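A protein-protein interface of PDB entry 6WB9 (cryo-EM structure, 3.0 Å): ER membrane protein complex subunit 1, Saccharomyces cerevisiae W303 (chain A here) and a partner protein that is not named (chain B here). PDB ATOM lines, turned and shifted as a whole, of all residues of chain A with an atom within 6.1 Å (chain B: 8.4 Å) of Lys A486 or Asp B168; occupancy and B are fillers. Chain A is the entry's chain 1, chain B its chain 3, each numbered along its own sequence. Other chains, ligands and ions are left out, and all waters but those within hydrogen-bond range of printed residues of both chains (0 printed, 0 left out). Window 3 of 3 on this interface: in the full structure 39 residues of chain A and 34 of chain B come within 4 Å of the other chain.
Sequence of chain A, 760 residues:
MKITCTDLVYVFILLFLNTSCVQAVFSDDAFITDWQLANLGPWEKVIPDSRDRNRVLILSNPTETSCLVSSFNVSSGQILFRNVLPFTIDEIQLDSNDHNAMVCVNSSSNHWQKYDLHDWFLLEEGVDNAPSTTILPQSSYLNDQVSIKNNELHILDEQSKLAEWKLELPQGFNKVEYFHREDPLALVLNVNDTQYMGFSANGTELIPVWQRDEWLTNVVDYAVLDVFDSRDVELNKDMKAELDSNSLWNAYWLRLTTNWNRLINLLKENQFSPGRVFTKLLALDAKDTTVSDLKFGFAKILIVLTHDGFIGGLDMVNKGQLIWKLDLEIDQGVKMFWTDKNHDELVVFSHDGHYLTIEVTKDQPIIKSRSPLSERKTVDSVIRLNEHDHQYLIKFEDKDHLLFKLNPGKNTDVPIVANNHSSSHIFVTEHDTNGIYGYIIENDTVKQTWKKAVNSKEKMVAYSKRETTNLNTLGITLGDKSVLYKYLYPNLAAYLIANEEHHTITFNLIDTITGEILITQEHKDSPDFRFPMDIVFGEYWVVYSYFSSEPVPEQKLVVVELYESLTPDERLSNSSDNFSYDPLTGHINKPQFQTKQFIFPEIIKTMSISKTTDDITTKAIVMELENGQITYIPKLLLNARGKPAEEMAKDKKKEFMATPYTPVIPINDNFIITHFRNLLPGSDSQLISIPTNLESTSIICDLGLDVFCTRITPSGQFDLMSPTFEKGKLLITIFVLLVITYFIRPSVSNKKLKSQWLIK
Gly A475 touches none of the printed residues of chain B.
Of chain B, only Asp B168 comes within 4 Å of Lys A486.
Printed residues of chain B within 4 Å of Ile A616: Cys B166 (2.8 Å), Asp B168 (3.3 Å) and Leu B169 (3.7 Å).
Printed residues of chain A within 4 Å of Cys B166: Ile A616 and Thr A617.
Of chain A, only Asn A472 (3.2 Å), Thr A473 (2.9 Å), Lys A486 (3.7 Å), Asp A615 (3.8 Å) and Ile A616 (3.3 Å) come within 4 Å of Asp B168.
Of the printed residues of chain A, Leu B169 touches Ile A616.
The nearest residue of chain B that does not touch Lys A486 is Gln B167 (6.6 Å).
ND2 of Asn A470 sits at hydrogen-bond distance from OD1 of Asn A472 (2.8 Å).
N of Asn A470 sits at hydrogen-bond distance from OD2 of Asp A615 (2.6 Å).
OG1 of Thr A473 lies within hydrogen-bond range of NZ of Lys A486, 2.8 Å away.
The backbone NH (N) of Lys A486 sits at hydrogen-bond distance from the backbone carbonyl oxygen (O) of Leu A474 (3.1 Å).
The side-chain carboxylate (OE1) of Glu A539 lies within salt-bridge range of the side-chain amino group (NZ) of Lys A486, 3.2 Å away.
O of Leu B169 lies close to NZ of Lys B157.
Asp A615 touches Asp B168 (O to OD2, 3.8 Å).
O of Ile A616 touches CB of Asp B168 (3.3 Å).
CG2 of Ile A616 touches CD2 of Leu B169, at 3.7 Å.
Of the 22 printed residues of chain A, 6 touch a printed residue of chain B.
Printed residues of chain A that touch a printed residue of chain B: Asn A472, Thr A473, Lys A486, Asp A615, Ile A616 and Thr A617.
Along chain A the printed residues that touch a printed residue of chain B span positions 472 to 617.
Hydrophobic or aromatic side chains of chain B that line the printed part of chain A: Leu B169.
Among the printed residues, Asp or Glu carboxylates within 4 Å of a Lys or Arg side-chain nitrogen of the other chain: Lys A486 with Asp B168.
The side-chain amide nitrogen (ND2) of Asn A472 lies within hydrogen-bond range of the side-chain carboxylate (OD2) of Asp B168 (3.2 Å).
The side-chain hydroxyl (OG1) of Thr A473 sits at hydrogen-bond distance from the side-chain carboxylate (OD1) of Asp B168 (2.9 Å).
OD1 of Asp B168 is in salt-bridge range of NZ of Lys A486 (3.7 Å).
The side-chain sulfur (SG) of Cys B166 lies within hydrogen-bond range of the backbone carbonyl oxygen (O) of Ile A616, at 2.8 Å.
The backbone NH (N) of Thr A617 lies close to the side-chain sulfur (SG) of Cys B166 (3.6 Å).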
ATOM      1  N   ASN A 470     -29.862  32.797  24.849  1.00  0.00           N
ATOM      2  CA  ASN A 470     -29.234  32.132  25.979  1.00  0.00           C
ATOM      3  C   ASN A 470     -27.968  31.429  25.513  1.00  0.00           C
ATOM      4  O   ASN A 470     -27.976  30.730  24.496  1.00  0.00           O
ATOM      5  CB  ASN A 470     -30.204  31.137  26.611  1.00  0.00           C
ATOM      6  CG  ASN A 470     -29.563  30.307  27.696  1.00  0.00           C
ATOM      7  OD1 ASN A 470     -29.343  30.783  28.807  1.00  0.00           O
ATOM      8  ND2 ASN A 470     -29.271  29.051  27.384  1.00  0.00           N
ATOM      9  N   LEU A 471     -26.878  31.619  26.251  1.00  0.00           N
ATOM     10  CA  LEU A 471     -25.583  31.078  25.861  1.00  0.00           C
ATOM     11  C   LEU A 471     -25.453  29.640  26.343  1.00  0.00           C
ATOM     12  O   LEU A 471     -25.587  29.363  27.539  1.00  0.00           O
ATOM     13  CB  LEU A 471     -24.444  31.927  26.418  1.00  0.00           C
ATOM     14  CG  LEU A 471     -23.059  31.376  26.081  1.00  0.00           C
ATOM     15  CD1 LEU A 471     -22.885  31.269  24.588  1.00  0.00           C
ATOM     16  CD2 LEU A 471     -21.992  32.253  26.651  1.00  0.00           C
ATOM     17  N   ASN A 472     -25.175  28.734  25.411  1.00  0.00           N
ATOM     18  CA  ASN A 472     -24.951  27.330  25.715  1.00  0.00           C
ATOM     19  C   ASN A 472     -23.518  26.897  25.451  1.00  0.00           C
ATOM     20  O   ASN A 472     -22.893  26.271  26.311  1.00  0.00           O
ATOM     21  CB  ASN A 472     -25.920  26.462  24.904  1.00  0.00           C
ATOM     22  CG  ASN A 472     -27.316  27.039  24.869  1.00  0.00           C
ATOM     23  OD1 ASN A 472     -27.995  27.116  25.891  1.00  0.00           O
ATOM     24  ND2 ASN A 472     -27.756  27.443  23.687  1.00  0.00           N
ATOM     25  N   THR A 473     -22.977  27.216  24.278  1.00  0.00           N
ATOM     26  CA  THR A 473     -21.604  26.888  23.927  1.00  0.00           C
ATOM     27  C   THR A 473     -20.861  28.152  23.521  1.00  0.00           C
ATOM     28  O   THR A 473     -21.373  28.960  22.741  1.00  0.00           O
ATOM     29  CB  THR A 473     -21.543  25.870  22.784  1.00  0.00           C
ATOM     30  OG1 THR A 473     -22.327  26.337  21.681  1.00  0.00           O
ATOM     31  CG2 THR A 473     -22.070  24.522  23.235  1.00  0.00           C
ATOM     32  N   LEU A 474     -19.645  28.308  24.043  1.00  0.00           N
ATOM     33  CA  LEU A 474     -18.831  29.481  23.752  1.00  0.00           C
ATOM     34  C   LEU A 474     -18.255  29.465  22.345  1.00  0.00           C
ATOM     35  O   LEU A 474     -17.869  30.521  21.839  1.00  0.00           O
ATOM     36  CB  LEU A 474     -17.679  29.595  24.754  1.00  0.00           C
ATOM     37  CG  LEU A 474     -17.806  30.367  26.072  1.00  0.00           C
ATOM     38  CD1 LEU A 474     -18.015  31.843  25.827  1.00  0.00           C
ATOM     39  CD2 LEU A 474     -18.907  29.815  26.960  1.00  0.00           C
ATOM     40  N   GLY A 475     -18.177  28.304  21.710  1.00  0.00           N
ATOM     41  CA  GLY A 475     -17.603  28.221  20.390  1.00  0.00           C
ATOM     42  C   GLY A 475     -18.015  26.948  19.691  1.00  0.00           C
ATOM     43  O   GLY A 475     -18.841  26.182  20.189  1.00  0.00           O
ATOM     44  N   ILE A 476     -17.423  26.729  18.521  1.00  0.00           N
ATOM     45  CA  ILE A 476     -17.718  25.576  17.678  1.00  0.00           C
ATOM     46  C   ILE A 476     -16.521  24.637  17.720  1.00  0.00           C
ATOM     47  O   ILE A 476     -15.410  25.019  17.336  1.00  0.00           O
ATOM     48  CB  ILE A 476     -18.047  25.992  16.234  1.00  0.00           C
ATOM     49  CG1 ILE A 476     -19.434  26.625  16.153  1.00  0.00           C
ATOM     50  CG2 ILE A 476     -17.991  24.802  15.302  1.00  0.00           C
ATOM     51  CD1 ILE A 476     -19.423  28.120  16.170  1.00  0.00           C
ATOM     52  N   VAL A 483     -11.459  24.793  19.014  1.00  0.00           N
ATOM     53  CA  VAL A 483     -12.640  25.639  19.106  1.00  0.00           C
ATOM     54  C   VAL A 483     -12.484  26.846  18.192  1.00  0.00           C
ATOM     55  O   VAL A 483     -11.457  27.533  18.220  1.00  0.00           O
ATOM     56  CB  VAL A 483     -12.874  26.076  20.558  1.00  0.00           C
ATOM     57  CG1 VAL A 483     -14.107  26.935  20.665  1.00  0.00           C
ATOM     58  CG2 VAL A 483     -13.006  24.872  21.442  1.00  0.00           C
ATOM     59  N   LEU A 484     -13.499  27.095  17.368  1.00  0.00           N
ATOM     60  CA  LEU A 484     -13.706  28.398  16.749  1.00  0.00           C
ATOM     61  C   LEU A 484     -14.687  29.162  17.625  1.00  0.00           C
ATOM     62  O   LEU A 484     -15.876  28.837  17.664  1.00  0.00           O
ATOM     63  CB  LEU A 484     -14.239  28.259  15.327  1.00  0.00           C
ATOM     64  CG  LEU A 484     -13.197  28.196  14.219  1.00  0.00           C
ATOM     65  CD1 LEU A 484     -13.879  28.097  12.887  1.00  0.00           C
ATOM     66  CD2 LEU A 484     -12.325  29.421  14.266  1.00  0.00           C
ATOM     67  N   TYR A 485     -14.194  30.172  18.329  1.00  0.00           N
ATOM     68  CA  TYR A 485     -15.001  30.861  19.323  1.00  0.00           C
ATOM     69  C   TYR A 485     -15.948  31.837  18.647  1.00  0.00           C
ATOM     70  O   TYR A 485     -15.543  32.595  17.764  1.00  0.00           O
ATOM     71  CB  TYR A 485     -14.104  31.588  20.319  1.00  0.00           C
ATOM     72  CG  TYR A 485     -13.352  30.654  21.233  1.00  0.00           C
ATOM     73  CD1 TYR A 485     -13.893  30.265  22.448  1.00  0.00           C
ATOM     74  CD2 TYR A 485     -12.109  30.152  20.877  1.00  0.00           C
ATOM     75  CE1 TYR A 485     -13.216  29.411  23.284  1.00  0.00           C
ATOM     76  CE2 TYR A 485     -11.423  29.296  21.706  1.00  0.00           C
ATOM     77  CZ  TYR A 485     -11.982  28.931  22.909  1.00  0.00           C
ATOM     78  OH  TYR A 485     -11.308  28.078  23.745  1.00  0.00           O
ATOM     79  N   LYS A 486     -17.210  31.809  19.061  1.00  0.00           N
ATOM     80  CA  LYS A 486     -18.211  32.694  18.490  1.00  0.00           C
ATOM     81  C   LYS A 486     -17.981  34.119  18.963  1.00  0.00           C
ATOM     82  O   LYS A 486     -17.463  34.358  20.054  1.00  0.00           O
ATOM     83  CB  LYS A 486     -19.612  32.243  18.890  1.00  0.00           C
ATOM     84  CG  LYS A 486     -19.857  30.762  18.766  1.00  0.00           C
ATOM     85  CD  LYS A 486     -21.157  30.376  19.435  1.00  0.00           C
ATOM     86  CE  LYS A 486     -21.451  28.906  19.263  1.00  0.00           C
ATOM     87  NZ  LYS A 486     -22.725  28.535  19.918  1.00  0.00           N
ATOM     88  N   TYR A 487     -18.368  35.075  18.126  1.00  0.00           N
ATOM     89  CA  TYR A 487     -18.315  36.480  18.517  1.00  0.00           C
ATOM     90  C   TYR A 487     -19.583  36.777  19.299  1.00  0.00           C
ATOM     91  O   TYR A 487     -20.575  37.270  18.764  1.00  0.00           O
ATOM     92  CB  TYR A 487     -18.169  37.387  17.306  1.00  0.00           C
ATOM     93  CG  TYR A 487     -17.862  38.811  17.677  1.00  0.00           C
ATOM     94  CD1 TYR A 487     -16.704  39.125  18.369  1.00  0.00           C
ATOM     95  CD2 TYR A 487     -18.727  39.841  17.345  1.00  0.00           C
ATOM     96  CE1 TYR A 487     -16.418  40.415  18.720  1.00  0.00           C
ATOM     97  CE2 TYR A 487     -18.446  41.141  17.691  1.00  0.00           C
ATOM     98  CZ  TYR A 487     -17.288  41.424  18.378  1.00  0.00           C
ATOM     99  OH  TYR A 487     -16.995  42.717  18.729  1.00  0.00           O
ATOM    100  N   LEU A 488     -19.544  36.470  20.595  1.00  0.00           N
ATOM    101  CA  LEU A 488     -20.692  36.615  21.479  1.00  0.00           C
ATOM    102  C   LEU A 488     -20.750  37.976  22.137  1.00  0.00           C
ATOM    103  O   LEU A 488     -21.330  38.111  23.222  1.00  0.00           O
ATOM    104  CB  LEU A 488     -20.672  35.524  22.543  1.00  0.00           C
ATOM    105  CG  LEU A 488     -20.599  34.113  21.989  1.00  0.00           C
ATOM    106  CD1 LEU A 488     -20.130  33.180  23.063  1.00  0.00           C
ATOM    107  CD2 LEU A 488     -21.946  33.699  21.466  1.00  0.00           C
ATOM    108  N   TYR A 489     -20.149  38.976  21.529  1.00  0.00           N
ATOM    109  CA  TYR A 489     -20.260  40.325  22.035  1.00  0.00           C
ATOM    110  C   TYR A 489     -21.669  40.828  21.771  1.00  0.00           C
ATOM    111  O   TYR A 489     -22.103  40.843  20.615  1.00  0.00           O
ATOM    112  CB  TYR A 489     -19.221  41.224  21.380  1.00  0.00           C
ATOM    113  CG  TYR A 489     -19.479  42.700  21.530  1.00  0.00           C
ATOM    114  CD1 TYR A 489     -19.527  43.298  22.780  1.00  0.00           C
ATOM    115  CD2 TYR A 489     -19.647  43.501  20.417  1.00  0.00           C
ATOM    116  CE1 TYR A 489     -19.757  44.646  22.916  1.00  0.00           C
ATOM    117  CE2 TYR A 489     -19.875  44.845  20.542  1.00  0.00           C
ATOM    118  CZ  TYR A 489     -19.932  45.414  21.795  1.00  0.00           C
ATOM    119  OH  TYR A 489     -20.159  46.762  21.924  1.00  0.00           O
ATOM    120  N   GLU A 539     -27.333  34.332  17.261  1.00  0.00           N
ATOM    121  CA  GLU A 539     -26.453  34.469  18.412  1.00  0.00           C
ATOM    122  C   GLU A 539     -25.112  35.060  18.009  1.00  0.00           C
ATOM    123  O   GLU A 539     -24.572  35.929  18.702  1.00  0.00           O
ATOM    124  CB  GLU A 539     -26.262  33.104  19.067  1.00  0.00           C
ATOM    125  CG  GLU A 539     -25.396  33.108  20.295  1.00  0.00           C
ATOM    126  CD  GLU A 539     -25.042  31.710  20.742  1.00  0.00           C
ATOM    127  OE1 GLU A 539     -24.952  30.816  19.875  1.00  0.00           O
ATOM    128  OE2 GLU A 539     -24.863  31.500  21.956  1.00  0.00           O
ATOM    129  N   TYR A 540     -24.563  34.597  16.892  1.00  0.00           N
ATOM    130  CA  TYR A 540     -23.263  35.045  16.415  1.00  0.00           C
ATOM    131  C   TYR A 540     -23.255  35.213  14.903  1.00  0.00           C
ATOM    132  O   TYR A 540     -22.180  35.267  14.304  1.00  0.00           O
ATOM    133  CB  TYR A 540     -22.156  34.062  16.832  1.00  0.00           C
ATOM    134  CG  TYR A 540     -22.259  32.677  16.218  1.00  0.00           C
ATOM    135  CD1 TYR A 540     -23.137  31.729  16.729  1.00  0.00           C
ATOM    136  CD2 TYR A 540     -21.458  32.308  15.145  1.00  0.00           C
ATOM    137  CE1 TYR A 540     -23.228  30.473  16.177  1.00  0.00           C
ATOM    138  CE2 TYR A 540     -21.547  31.055  14.586  1.00  0.00           C
ATOM    139  CZ  TYR A 540     -22.432  30.143  15.108  1.00  0.00           C
ATOM    140  OH  TYR A 540     -22.521  28.888  14.555  1.00  0.00           O
ATOM    141  N   LEU A 562     -19.979  35.415  12.600  1.00  0.00           N
ATOM    142  CA  LEU A 562     -18.976  36.245  13.255  1.00  0.00           C
ATOM    143  C   LEU A 562     -18.274  35.420  14.320  1.00  0.00           C
ATOM    144  O   LEU A 562     -18.926  34.882  15.219  1.00  0.00           O
ATOM    145  CB  LEU A 562     -19.613  37.483  13.886  1.00  0.00           C
ATOM    146  CG  LEU A 562     -19.843  38.721  13.024  1.00  0.00           C
ATOM    147  CD1 LEU A 562     -20.869  38.429  11.959  1.00  0.00           C
ATOM    148  CD2 LEU A 562     -20.282  39.881  13.868  1.00  0.00           C
ATOM    149  N   TYR A 563     -16.951  35.327  14.225  1.00  0.00           N
ATOM    150  CA  TYR A 563     -16.121  34.638  15.195  1.00  0.00           C
ATOM    151  C   TYR A 563     -15.120  35.623  15.779  1.00  0.00           C
ATOM    152  O   TYR A 563     -14.918  36.718  15.256  1.00  0.00           O
ATOM    153  CB  TYR A 563     -15.402  33.453  14.547  1.00  0.00           C
ATOM    154  CG  TYR A 563     -16.350  32.474  13.915  1.00  0.00           C
ATOM    155  CD1 TYR A 563     -17.053  31.572  14.693  1.00  0.00           C
ATOM    156  CD2 TYR A 563     -16.557  32.462  12.545  1.00  0.00           C
ATOM    157  CE1 TYR A 563     -17.927  30.683  14.130  1.00  0.00           C
ATOM    158  CE2 TYR A 563     -17.435  31.575  11.970  1.00  0.00           C
ATOM    159  CZ  TYR A 563     -18.115  30.687  12.771  1.00  0.00           C
ATOM    160  OH  TYR A 563     -18.995  29.791  12.219  1.00  0.00           O
ATOM    161  N   GLU A 564     -14.498  35.231  16.889  1.00  0.00           N
ATOM    162  CA  GLU A 564     -13.471  36.082  17.477  1.00  0.00           C
ATOM    163  C   GLU A 564     -12.198  36.059  16.649  1.00  0.00           C
ATOM    164  O   GLU A 564     -11.501  37.075  16.556  1.00  0.00           O
ATOM    165  CB  GLU A 564     -13.186  35.648  18.908  1.00  0.00           C
ATOM    166  CG  GLU A 564     -14.291  36.010  19.861  1.00  0.00           C
ATOM    167  CD  GLU A 564     -14.115  35.363  21.201  1.00  0.00           C
ATOM    168  OE1 GLU A 564     -13.143  34.603  21.353  1.00  0.00           O
ATOM    169  OE2 GLU A 564     -14.945  35.608  22.100  1.00  0.00           O
ATOM    170  N   ASP A 615     -32.598  28.131  24.061  1.00  0.00           N
ATOM    171  CA  ASP A 615     -31.911  28.338  22.779  1.00  0.00           C
ATOM    172  C   ASP A 615     -30.912  27.220  22.489  1.00  0.00           C
ATOM    173  O   ASP A 615     -29.826  27.452  21.957  1.00  0.00           O
ATOM    174  CB  ASP A 615     -31.241  29.712  22.717  1.00  0.00           C
ATOM    175  CG  ASP A 615     -32.227  30.847  22.903  1.00  0.00           C
ATOM    176  OD1 ASP A 615     -33.216  30.912  22.147  1.00  0.00           O
ATOM    177  OD2 ASP A 615     -32.019  31.673  23.815  1.00  0.00           O
ATOM    178  N   ILE A 616     -31.292  25.994  22.842  1.00  0.00           N
ATOM    179  CA  ILE A 616     -30.415  24.844  22.653  1.00  0.00           C
ATOM    180  C   ILE A 616     -30.463  24.368  21.210  1.00  0.00           C
ATOM    181  O   ILE A 616     -29.435  24.301  20.528  1.00  0.00           O
ATOM    182  CB  ILE A 616     -30.798  23.709  23.622  1.00  0.00           C
ATOM    183  CG1 ILE A 616     -30.546  24.110  25.078  1.00  0.00           C
ATOM    184  CG2 ILE A 616     -30.065  22.435  23.257  1.00  0.00           C
ATOM    185  CD1 ILE A 616     -29.114  24.020  25.508  1.00  0.00           C
ATOM    186  N   THR A 617     -31.661  24.043  20.725  1.00  0.00           N
ATOM    187  CA  THR A 617     -31.833  23.484  19.393  1.00  0.00           C
ATOM    188  C   THR A 617     -31.500  24.515  18.319  1.00  0.00           C
ATOM    189  O   THR A 617     -31.388  25.713  18.589  1.00  0.00           O
ATOM    190  CB  THR A 617     -33.258  22.967  19.208  1.00  0.00           C
ATOM    191  OG1 THR A 617     -33.349  22.237  17.980  1.00  0.00           O
ATOM    192  CG2 THR A 617     -34.225  24.108  19.173  1.00  0.00           C
ATOM    193  N   MET B   1     -33.885  21.376  30.794  1.00  0.00           N
ATOM    194  CA  MET B   1     -34.630  20.945  29.616  1.00  0.00           C
ATOM    195  C   MET B   1     -35.765  20.004  29.996  1.00  0.00           C
ATOM    196  O   MET B   1     -35.548  18.980  30.638  1.00  0.00           O
ATOM    197  CB  MET B   1     -33.697  20.273  28.613  1.00  0.00           C
ATOM    198  CG  MET B   1     -34.407  19.533  27.500  1.00  0.00           C
ATOM    199  SD  MET B   1     -33.240  18.870  26.309  1.00  0.00           S
ATOM    200  CE  MET B   1     -32.340  20.359  25.921  1.00  0.00           C
ATOM    201  N   LYS B 157     -20.525  13.237  22.203  1.00  0.00           N
ATOM    202  CA  LYS B 157     -21.689  13.726  21.470  1.00  0.00           C
ATOM    203  C   LYS B 157     -21.827  13.048  20.112  1.00  0.00           C
ATOM    204  O   LYS B 157     -22.939  12.939  19.585  1.00  0.00           O
ATOM    205  CB  LYS B 157     -21.589  15.238  21.288  1.00  0.00           C
ATOM    206  CG  LYS B 157     -22.910  15.969  21.366  1.00  0.00           C
ATOM    207  CD  LYS B 157     -22.750  17.436  21.013  1.00  0.00           C
ATOM    208  CE  LYS B 157     -21.726  18.107  21.906  1.00  0.00           C
ATOM    209  NZ  LYS B 157     -21.708  19.579  21.717  1.00  0.00           N
ATOM    210  N   GLN B 161     -25.434  10.876  21.170  1.00  0.00           N
ATOM    211  CA  GLN B 161     -26.554  11.524  20.498  1.00  0.00           C
ATOM    212  C   GLN B 161     -26.491  11.156  19.024  1.00  0.00           C
ATOM    213  O   GLN B 161     -25.498  11.455  18.352  1.00  0.00           O
ATOM    214  CB  GLN B 161     -26.504  13.040  20.674  1.00  0.00           C
ATOM    215  CG  GLN B 161     -26.419  13.493  22.111  1.00  0.00           C
ATOM    216  CD  GLN B 161     -26.268  14.990  22.239  1.00  0.00           C
ATOM    217  OE1 GLN B 161     -26.251  15.707  21.245  1.00  0.00           O
ATOM    218  NE2 GLN B 161     -26.162  15.470  23.468  1.00  0.00           N
ATOM    219  N   ILE B 164     -29.976  13.534  16.559  1.00  0.00           N
ATOM    220  CA  ILE B 164     -30.068  14.943  16.920  1.00  0.00           C
ATOM    221  C   ILE B 164     -28.774  15.616  16.488  1.00  0.00           C
ATOM    222  O   ILE B 164     -27.700  15.293  17.009  1.00  0.00           O
ATOM    223  CB  ILE B 164     -30.303  15.146  18.427  1.00  0.00           C
ATOM    224  CG1 ILE B 164     -31.647  14.555  18.863  1.00  0.00           C
ATOM    225  CG2 ILE B 164     -30.254  16.618  18.773  1.00  0.00           C
ATOM    226  CD1 ILE B 164     -31.554  13.173  19.480  1.00  0.00           C
ATOM    227  N   ILE B 165     -28.874  16.547  15.540  1.00  0.00           N
ATOM    228  CA  ILE B 165     -27.702  17.208  14.974  1.00  0.00           C
ATOM    229  C   ILE B 165     -27.479  18.556  15.646  1.00  0.00           C
ATOM    230  O   ILE B 165     -26.662  19.360  15.182  1.00  0.00           O
ATOM    231  CB  ILE B 165     -27.832  17.373  13.448  1.00  0.00           C
ATOM    232  CG1 ILE B 165     -29.050  18.238  13.093  1.00  0.00           C
ATOM    233  CG2 ILE B 165     -27.887  16.013  12.771  1.00  0.00           C
ATOM    234  CD1 ILE B 165     -29.129  18.628  11.630  1.00  0.00           C
ATOM    235  N   CYS B 166     -28.209  18.814  16.728  1.00  0.00           N
ATOM    236  CA  CYS B 166     -28.075  20.068  17.458  1.00  0.00           C
ATOM    237  C   CYS B 166     -26.714  20.152  18.139  1.00  0.00           C
ATOM    238  O   CYS B 166     -26.287  19.216  18.820  1.00  0.00           O
ATOM    239  CB  CYS B 166     -29.197  20.193  18.486  1.00  0.00           C
ATOM    240  SG  CYS B 166     -29.200  21.734  19.398  1.00  0.00           S
ATOM    241  N   GLN B 167     -26.032  21.280  17.950  1.00  0.00           N
ATOM    242  CA  GLN B 167     -24.655  21.443  18.395  1.00  0.00           C
ATOM    243  C   GLN B 167     -24.527  22.053  19.783  1.00  0.00           C
ATOM    244  O   GLN B 167     -23.454  21.953  20.384  1.00  0.00           O
ATOM    245  CB  GLN B 167     -23.882  22.313  17.399  1.00  0.00           C
ATOM    246  CG  GLN B 167     -23.949  21.823  15.968  1.00  0.00           C
ATOM    247  CD  GLN B 167     -23.150  22.693  15.019  1.00  0.00           C
ATOM    248  OE1 GLN B 167     -22.892  23.864  15.297  1.00  0.00           O
ATOM    249  NE2 GLN B 167     -22.748  22.120  13.893  1.00  0.00           N
ATOM    250  N   ASP B 168     -25.574  22.688  20.301  1.00  0.00           N
ATOM    251  CA  ASP B 168     -25.528  23.299  21.621  1.00  0.00           C
ATOM    252  C   ASP B 168     -25.994  22.359  22.720  1.00  0.00           C
ATOM    253  O   ASP B 168     -25.969  22.740  23.893  1.00  0.00           O
ATOM    254  CB  ASP B 168     -26.366  24.579  21.647  1.00  0.00           C
ATOM    255  CG  ASP B 168     -25.734  25.705  20.855  1.00  0.00           C
ATOM    256  OD1 ASP B 168     -24.692  25.471  20.209  1.00  0.00           O
ATOM    257  OD2 ASP B 168     -26.275  26.829  20.881  1.00  0.00           O
ATOM    258  N   LEU B 169     -26.424  21.152  22.369  1.00  0.00           N
ATOM    259  CA  LEU B 169     -26.695  20.124  23.364  1.00  0.00           C
ATOM    260  C   LEU B 169     -25.381  19.641  23.953  1.00  0.00           C
ATOM    261  O   LEU B 169     -24.560  19.062  23.239  1.00  0.00           O
ATOM    262  CB  LEU B 169     -27.441  18.957  22.726  1.00  0.00           C
ATOM    263  CG  LEU B 169     -28.952  18.876  22.898  1.00  0.00           C
ATOM    264  CD1 LEU B 169     -29.474  17.604  22.287  1.00  0.00           C
ATOM    265  CD2 LEU B 169     -29.298  18.936  24.353  1.00  0.00           C
ATOM    266  N   ASP B 170     -25.172  19.874  25.245  1.00  0.00           N
ATOM    267  CA  ASP B 170     -23.963  19.361  25.867  1.00  0.00           C
ATOM    268  C   ASP B 170     -24.093  17.859  26.079  1.00  0.00           C
ATOM    269  O   ASP B 170     -25.183  17.288  25.996  1.00  0.00           O
ATOM    270  CB  ASP B 170     -23.683  20.066  27.191  1.00  0.00           C
ATOM    271  CG  ASP B 170     -24.655  19.674  28.275  1.00  0.00           C
ATOM    272  OD1 ASP B 170     -25.867  19.626  27.994  1.00  0.00           O
ATOM    273  OD2 ASP B 170     -24.207  19.412  29.409  1.00  0.00           O
ATOM    274  N   VAL B 171     -22.970  17.207  26.361  1.00  0.00           N
ATOM    275  CA  VAL B 171     -22.964  15.743  26.487  1.00  0.00           C
ATOM    276  C   VAL B 171     -23.289  15.444  27.942  1.00  0.00           C
ATOM    277  O   VAL B 171     -22.440  15.076  28.757  1.00  0.00           O
ATOM    278  CB  VAL B 171     -21.639  15.132  26.041  1.00  0.00           C
ATOM    279  CG1 VAL B 171     -21.643  13.643  26.306  1.00  0.00           C
ATOM    280  CG2 VAL B 171     -21.426  15.413  24.590  1.00  0.00           C
ATOM    281  N   TRP B 173     -27.242  15.269  27.873  1.00  0.00           N
ATOM    282  CA  TRP B 173     -28.490  14.883  27.238  1.00  0.00           C
ATOM    283  C   TRP B 173     -28.183  13.908  26.117  1.00  0.00           C
ATOM    284  O   TRP B 173     -27.519  14.263  25.139  1.00  0.00           O
ATOM    285  CB  TRP B 173     -29.218  16.113  26.713  1.00  0.00           C
ATOM    286  CG  TRP B 173     -29.429  17.135  27.761  1.00  0.00           C
ATOM    287  CD1 TRP B 173     -28.655  18.223  28.004  1.00  0.00           C
ATOM    288  CD2 TRP B 173     -30.478  17.163  28.730  1.00  0.00           C
ATOM    289  NE1 TRP B 173     -29.156  18.935  29.062  1.00  0.00           N
ATOM    290  CE2 TRP B 173     -30.278  18.302  29.526  1.00  0.00           C
ATOM    291  CE3 TRP B 173     -31.568  16.335  29.001  1.00  0.00           C
ATOM    292  CZ2 TRP B 173     -31.126  18.636  30.573  1.00  0.00           C
ATOM    293  CZ3 TRP B 173     -32.407  16.668  30.039  1.00  0.00           C
ATOM    294  CH2 TRP B 173     -32.184  17.807  30.813  1.00  0.00           C
